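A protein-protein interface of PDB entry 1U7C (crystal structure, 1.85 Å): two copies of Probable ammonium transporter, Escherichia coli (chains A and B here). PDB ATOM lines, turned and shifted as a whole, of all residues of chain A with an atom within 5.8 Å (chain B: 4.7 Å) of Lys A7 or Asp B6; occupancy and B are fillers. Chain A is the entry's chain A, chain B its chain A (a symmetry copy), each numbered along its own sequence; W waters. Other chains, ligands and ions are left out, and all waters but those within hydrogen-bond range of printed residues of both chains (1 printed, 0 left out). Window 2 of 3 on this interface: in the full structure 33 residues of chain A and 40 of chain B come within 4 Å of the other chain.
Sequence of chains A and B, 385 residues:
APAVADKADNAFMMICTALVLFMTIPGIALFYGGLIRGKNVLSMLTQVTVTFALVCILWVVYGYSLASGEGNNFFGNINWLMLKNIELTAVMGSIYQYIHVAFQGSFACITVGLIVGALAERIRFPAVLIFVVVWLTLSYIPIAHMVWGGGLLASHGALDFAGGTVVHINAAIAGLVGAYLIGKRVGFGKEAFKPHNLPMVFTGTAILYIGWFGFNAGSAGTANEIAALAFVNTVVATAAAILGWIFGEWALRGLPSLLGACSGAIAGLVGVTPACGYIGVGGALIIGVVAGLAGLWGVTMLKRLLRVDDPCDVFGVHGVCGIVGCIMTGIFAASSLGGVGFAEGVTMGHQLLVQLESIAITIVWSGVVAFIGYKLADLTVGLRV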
ATOM      1  N   ALA A   5     -18.358  27.675   8.473  1.00  0.00           N
ATOM      2  CA  ALA A   5     -19.277  26.607   8.118  1.00  0.00           C
ATOM      3  C   ALA A   5     -20.738  26.991   8.307  1.00  0.00           C
ATOM      4  O   ALA A   5     -21.099  27.678   9.263  1.00  0.00           O
ATOM      5  CB  ALA A   5     -18.963  25.361   8.939  1.00  0.00           C
ATOM      6  N   ASP A   6     -21.571  26.544   7.375  1.00  0.00           N
ATOM      7  CA  ASP A   6     -23.002  26.788   7.432  1.00  0.00           C
ATOM      8  C   ASP A   6     -23.544  25.487   8.015  1.00  0.00           C
ATOM      9  O   ASP A   6     -23.374  24.422   7.415  1.00  0.00           O
ATOM     10  CB  ASP A   6     -23.554  27.012   6.023  1.00  0.00           C
ATOM     11  CG  ASP A   6     -25.049  27.252   6.013  1.00  0.00           C
ATOM     12  OD1 ASP A   6     -25.471  28.404   5.775  1.00  0.00           O
ATOM     13  OD2 ASP A   6     -25.803  26.286   6.247  1.00  0.00           O
ATOM     14  N   LYS A   7     -24.172  25.558   9.183  1.00  0.00           N
ATOM     15  CA  LYS A   7     -24.690  24.349   9.809  1.00  0.00           C
ATOM     16  C   LYS A   7     -25.714  23.611   8.971  1.00  0.00           C
ATOM     17  O   LYS A   7     -25.807  22.388   9.052  1.00  0.00           O
ATOM     18  CB  LYS A   7     -25.249  24.656  11.200  1.00  0.00           C
ATOM     19  CG  LYS A   7     -24.151  25.000  12.197  1.00  0.00           C
ATOM     20  CD  LYS A   7     -24.597  24.820  13.642  1.00  0.00           C
ATOM     21  CE  LYS A   7     -25.640  25.839  14.043  1.00  0.00           C
ATOM     22  NZ  LYS A   7     -25.954  25.735  15.497  1.00  0.00           N
ATOM     23  N   ALA A   8     -26.481  24.340   8.168  1.00  0.00           N
ATOM     24  CA  ALA A   8     -27.470  23.702   7.305  1.00  0.00           C
ATOM     25  C   ALA A   8     -26.724  22.828   6.308  1.00  0.00           C
ATOM     26  O   ALA A   8     -27.130  21.702   6.031  1.00  0.00           O
ATOM     27  CB  ALA A   8     -28.294  24.749   6.564  1.00  0.00           C
ATOM     28  N   ASP A   9     -25.630  23.352   5.765  1.00  0.00           N
ATOM     29  CA  ASP A   9     -24.846  22.588   4.811  1.00  0.00           C
ATOM     30  C   ASP A   9     -24.153  21.433   5.519  1.00  0.00           C
ATOM     31  O   ASP A   9     -24.058  20.343   4.965  1.00  0.00           O
ATOM     32  CB  ASP A   9     -23.821  23.481   4.112  1.00  0.00           C
ATOM     33  CG  ASP A   9     -24.472  24.520   3.224  1.00  0.00           C
ATOM     34  OD1 ASP A   9     -25.614  24.295   2.779  1.00  0.00           O
ATOM     35  OD2 ASP A   9     -23.833  25.557   2.959  1.00  0.00           O
ATOM     36  N   ASN A  10     -23.666  21.664   6.740  1.00  0.00           N
ATOM     37  CA  ASN A  10     -23.023  20.591   7.496  1.00  0.00           C
ATOM     38  C   ASN A  10     -24.012  19.447   7.661  1.00  0.00           C
ATOM     39  O   ASN A  10     -23.682  18.282   7.439  1.00  0.00           O
ATOM     40  CB  ASN A  10     -22.628  21.038   8.902  1.00  0.00           C
ATOM     41  CG  ASN A  10     -21.448  21.973   8.920  1.00  0.00           C
ATOM     42  OD1 ASN A  10     -20.608  21.966   8.020  1.00  0.00           O
ATOM     43  ND2 ASN A  10     -21.364  22.773   9.971  1.00  0.00           N
ATOM     44  N   ALA A  11     -25.223  19.795   8.083  1.00  0.00           N
ATOM     45  CA  ALA A  11     -26.274  18.811   8.307  1.00  0.00           C
ATOM     46  C   ALA A  11     -26.592  18.087   7.010  1.00  0.00           C
ATOM     47  O   ALA A  11     -26.612  16.860   6.958  1.00  0.00           O
ATOM     48  CB  ALA A  11     -27.522  19.503   8.843  1.00  0.00           C
ATOM     49  N   PHE A  12     -26.841  18.858   5.959  1.00  0.00           N
ATOM     50  CA  PHE A  12     -27.159  18.282   4.665  1.00  0.00           C
ATOM     51  C   PHE A  12     -26.073  17.328   4.200  1.00  0.00           C
ATOM     52  O   PHE A  12     -26.349  16.206   3.778  1.00  0.00           O
ATOM     53  CB  PHE A  12     -27.315  19.387   3.625  1.00  0.00           C
ATOM     54  CG  PHE A  12     -27.686  18.893   2.260  1.00  0.00           C
ATOM     55  CD1 PHE A  12     -28.858  18.167   2.067  1.00  0.00           C
ATOM     56  CD2 PHE A  12     -26.880  19.174   1.162  1.00  0.00           C
ATOM     57  CE1 PHE A  12     -29.222  17.736   0.793  1.00  0.00           C
ATOM     58  CE2 PHE A  12     -27.237  18.747  -0.114  1.00  0.00           C
ATOM     59  CZ  PHE A  12     -28.410  18.027  -0.295  1.00  0.00           C
ATOM     60  N   SER A  94     -18.529  25.325   2.301  1.00  0.00           N
ATOM     61  CA  SER A  94     -19.363  25.900   3.345  1.00  0.00           C
ATOM     62  C   SER A  94     -19.637  24.892   4.453  1.00  0.00           C
ATOM     63  O   SER A  94     -20.552  25.067   5.253  1.00  0.00           O
ATOM     64  CB  SER A  94     -20.683  26.389   2.756  1.00  0.00           C
ATOM     65  OG  SER A  94     -21.359  25.337   2.097  1.00  0.00           O
ATOM     66  N   VAL B   4     -32.822  30.034  21.422  1.00  0.00           N
ATOM     67  CA  VAL B   4     -33.467  30.037  20.116  1.00  0.00           C
ATOM     68  C   VAL B   4     -32.981  28.845  19.303  1.00  0.00           C
ATOM     69  O   VAL B   4     -31.783  28.589  19.213  1.00  0.00           O
ATOM     70  CB  VAL B   4     -33.168  31.340  19.341  1.00  0.00           C
ATOM     71  CG1 VAL B   4     -33.634  31.208  17.898  1.00  0.00           C
ATOM     72  CG2 VAL B   4     -33.873  32.508  20.009  1.00  0.00           C
ATOM     73  N   ALA B   5     -33.921  28.117  18.714  1.00  0.00           N
ATOM     74  CA  ALA B   5     -33.582  26.943  17.928  1.00  0.00           C
ATOM     75  C   ALA B   5     -32.911  27.286  16.605  1.00  0.00           C
ATOM     76  O   ALA B   5     -33.269  28.259  15.942  1.00  0.00           O
ATOM     77  CB  ALA B   5     -34.835  26.114  17.669  1.00  0.00           C
ATOM     78  N   ASP B   6     -31.924  26.476  16.238  1.00  0.00           N
ATOM     79  CA  ASP B   6     -31.212  26.642  14.984  1.00  0.00           C
ATOM     80  C   ASP B   6     -31.889  25.624  14.073  1.00  0.00           C
ATOM     81  O   ASP B   6     -31.863  24.424  14.357  1.00  0.00           O
ATOM     82  CB  ASP B   6     -29.733  26.291  15.169  1.00  0.00           C
ATOM     83  CG  ASP B   6     -28.936  26.425  13.887  1.00  0.00           C
ATOM     84  OD1 ASP B   6     -28.137  27.378  13.774  1.00  0.00           O
ATOM     85  OD2 ASP B   6     -29.114  25.574  12.992  1.00  0.00           O
ATOM     86  N   LYS B   7     -32.512  26.090  12.996  1.00  0.00           N
ATOM     87  CA  LYS B   7     -33.204  25.175  12.098  1.00  0.00           C
ATOM     88  C   LYS B   7     -32.307  24.120  11.482  1.00  0.00           C
ATOM     89  O   LYS B   7     -32.764  23.014  11.206  1.00  0.00           O
ATOM     90  CB  LYS B   7     -33.956  25.947  11.012  1.00  0.00           C
ATOM     91  CG  LYS B   7     -35.155  26.701  11.569  1.00  0.00           C
ATOM     92  CD  LYS B   7     -36.177  27.049  10.495  1.00  0.00           C
ATOM     93  CE  LYS B   7     -35.649  28.082   9.525  1.00  0.00           C
ATOM     94  NZ  LYS B   7     -36.713  28.511   8.574  1.00  0.00           N
ATOM     95  N   ALA B   8     -31.039  24.452  11.267  1.00  0.00           N
ATOM     96  CA  ALA B   8     -30.103  23.482  10.706  1.00  0.00           C
ATOM     97  C   ALA B   8     -29.958  22.343  11.705  1.00  0.00           C
ATOM     98  O   ALA B   8     -29.944  21.174  11.327  1.00  0.00           O
ATOM     99  CB  ALA B   8     -28.744  24.128  10.454  1.00  0.00           C
ATOM    100  N   ASP B   9     -29.848  22.688  12.984  1.00  0.00           N
ATOM    101  CA  ASP B   9     -29.718  21.670  14.010  1.00  0.00           C
ATOM    102  C   ASP B   9     -31.025  20.904  14.148  1.00  0.00           C
ATOM    103  O   ASP B   9     -31.009  19.693  14.343  1.00  0.00           O
ATOM    104  CB  ASP B   9     -29.318  22.293  15.346  1.00  0.00           C
ATOM    105  CG  ASP B   9     -27.925  22.886  15.313  1.00  0.00           C
ATOM    106  OD1 ASP B   9     -27.109  22.447  14.480  1.00  0.00           O
ATOM    107  OD2 ASP B   9     -27.643  23.783  16.131  1.00  0.00           O
ATOM    108  N   ASN B  10     -32.158  21.602  14.051  1.00  0.00           N
ATOM    109  CA  ASN B  10     -33.453  20.927  14.134  1.00  0.00           C
ATOM    110  C   ASN B  10     -33.527  19.873  13.039  1.00  0.00           C
ATOM    111  O   ASN B  10     -33.917  18.730  13.279  1.00  0.00           O
ATOM    112  CB  ASN B  10     -34.616  21.888  13.899  1.00  0.00           C
ATOM    113  CG  ASN B  10     -34.853  22.828  15.050  1.00  0.00           C
ATOM    114  OD1 ASN B  10     -34.524  22.534  16.199  1.00  0.00           O
ATOM    115  ND2 ASN B  10     -35.458  23.967  14.750  1.00  0.00           N
ATOM    116  N   SER B  94     -29.689  23.626  21.072  1.00  0.00           N
ATOM    117  CA  SER B  94     -29.936  24.501  19.935  1.00  0.00           C
ATOM    118  C   SER B  94     -31.059  23.965  19.059  1.00  0.00           C
ATOM    119  O   SER B  94     -31.214  24.374  17.911  1.00  0.00           O
ATOM    120  CB  SER B  94     -28.665  24.658  19.104  1.00  0.00           C
ATOM    121  OG  SER B  94     -28.188  23.399  18.673  1.00  0.00           O
ATOM    122  N   THR B 222     -26.029  19.003  17.419  1.00  0.00           N
ATOM    123  CA  THR B 222     -25.932  20.091  16.464  1.00  0.00           C
ATOM    124  C   THR B 222     -25.076  19.624  15.301  1.00  0.00           C
ATOM    125  O   THR B 222     -24.223  18.756  15.463  1.00  0.00           O
ATOM    126  CB  THR B 222     -25.278  21.323  17.117  1.00  0.00           C
ATOM    127  OG1 THR B 222     -24.921  22.276  16.110  1.00  0.00           O
ATOM    128  CG2 THR B 222     -24.035  20.912  17.891  1.00  0.00           C
ATOM    129  N   ALA B 223     -25.314  20.195  14.127  1.00  0.00           N
ATOM    130  CA  ALA B 223     -24.545  19.827  12.953  1.00  0.00           C
ATOM    131  C   ALA B 223     -23.294  20.696  12.937  1.00  0.00           C
ATOM    132  O   ALA B 223     -23.144  21.577  12.090  1.00  0.00           O
ATOM    133  CB  ALA B 223     -25.372  20.057  11.703  1.00  0.00           C
HETATM  134  O   HOH W   1     -23.587  24.649  16.686  1.00  0.00           O
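Water W1 lies within hydrogen-bond range of the side-chain hydroxyl of Thr B222 and the side-chain amino group of Lys A7.
Of the printed residues of chain B, Lys A7 touches Asp B6, Ala B8, Asp B9, Thr B222 and Ala B223.
Asp B6 touches one residue of chain A.
Of the printed residues of chain B, Ala A11 touches Ala B8 and Ala B223.
Printed residues of chain A within 4 Å of Asp B9: Lys A7.
Of the printed residues of chain B, Ala A8 touches Ala B8.
Of the printed residues of chain A, Thr B222 touches Lys A7.
Of the printed residues of chain A, Ala B8 touches Lys A7 (3.4 Å), Ala A8 (3.2 Å) and Ala A11 (3.9 Å).
Asn B10 touches none of the printed residues of chain A.
The nearest residue of chain B that does not touch Lys A7 is Ser B94 (4.5 Å).
The nearest residue of chain A that does not touch Asp B6 is Ala A8 (5.6 Å).
Of the 9 printed residues of chain A, 4 touch a printed residue of chain B.
Hydrophobic or aromatic side chains of chain A that line the printed part of chain B: Ala A8 and Ala A11.
NZ of Lys A7 lies within salt-bridge range of OD1 of Asp B6, 3.2 Å away.
The side-chain amino group of Lys A7 is in salt-bridge range of the side-chain carboxylate of Asp B9 (2.7 Å).
The side-chain amide nitrogen (ND2) of Asn A10 lies within hydrogen-bond range of the backbone carbonyl oxygen (O) of Ala B223 (3.0 Å).
Ala B8 touches Lys A7.
Thr B222 touches Lys A7.
Ala B223 touches Lys A7 (CB to O, 3.6 Å).
CB of Ala B8 touches N of Ala A8, 3.2 Å away.
O of Ala B8 touches CB of Ala A11 (3.9 Å).
CB of Ala A11 touches CB of Ala B223, at 3.6 Å.
Lys A7 touches Asp B6, but with the chains exchanged Asp A6 does not touch Lys B7 (8.6 Å).
Lys A7 touches Ala B8, but with the chains exchanged Ala A8 does not touch Lys B7 (6.4 Å).
Lys A7 touches Asp B9, but with the chains exchanged Asp A9 does not touch Lys B7 (8.8 Å).
Ala A8 touches its own counterpart, Ala B8.
OD2 of Asp B6 lies within hydrogen-bond range of N of Ala B8, 2.8 Å away.
The backbone NH (N) of Asp B9 sits at hydrogen-bond distance from the side-chain carboxylate (OD2) of Asp B6, at 3.0 Å.
The backbone NH (N) of Asp B6 lies within hydrogen-bond range of the backbone carbonyl oxygen (O) of Ser B94 (2.8 Å).
The side-chain carboxylate of Asp B9 sits at hydrogen-bond distance from the side-chain hydroxyl of Ser B94 (2.6 Å).
The side-chain hydroxyl of Thr B222 is in hydrogen-bond range of the side-chain carboxylate of Asp B9 (2.7 Å).
OD1 of Asp B9 is in hydrogen-bond range of N of Ala B223, at 2.9 Å.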
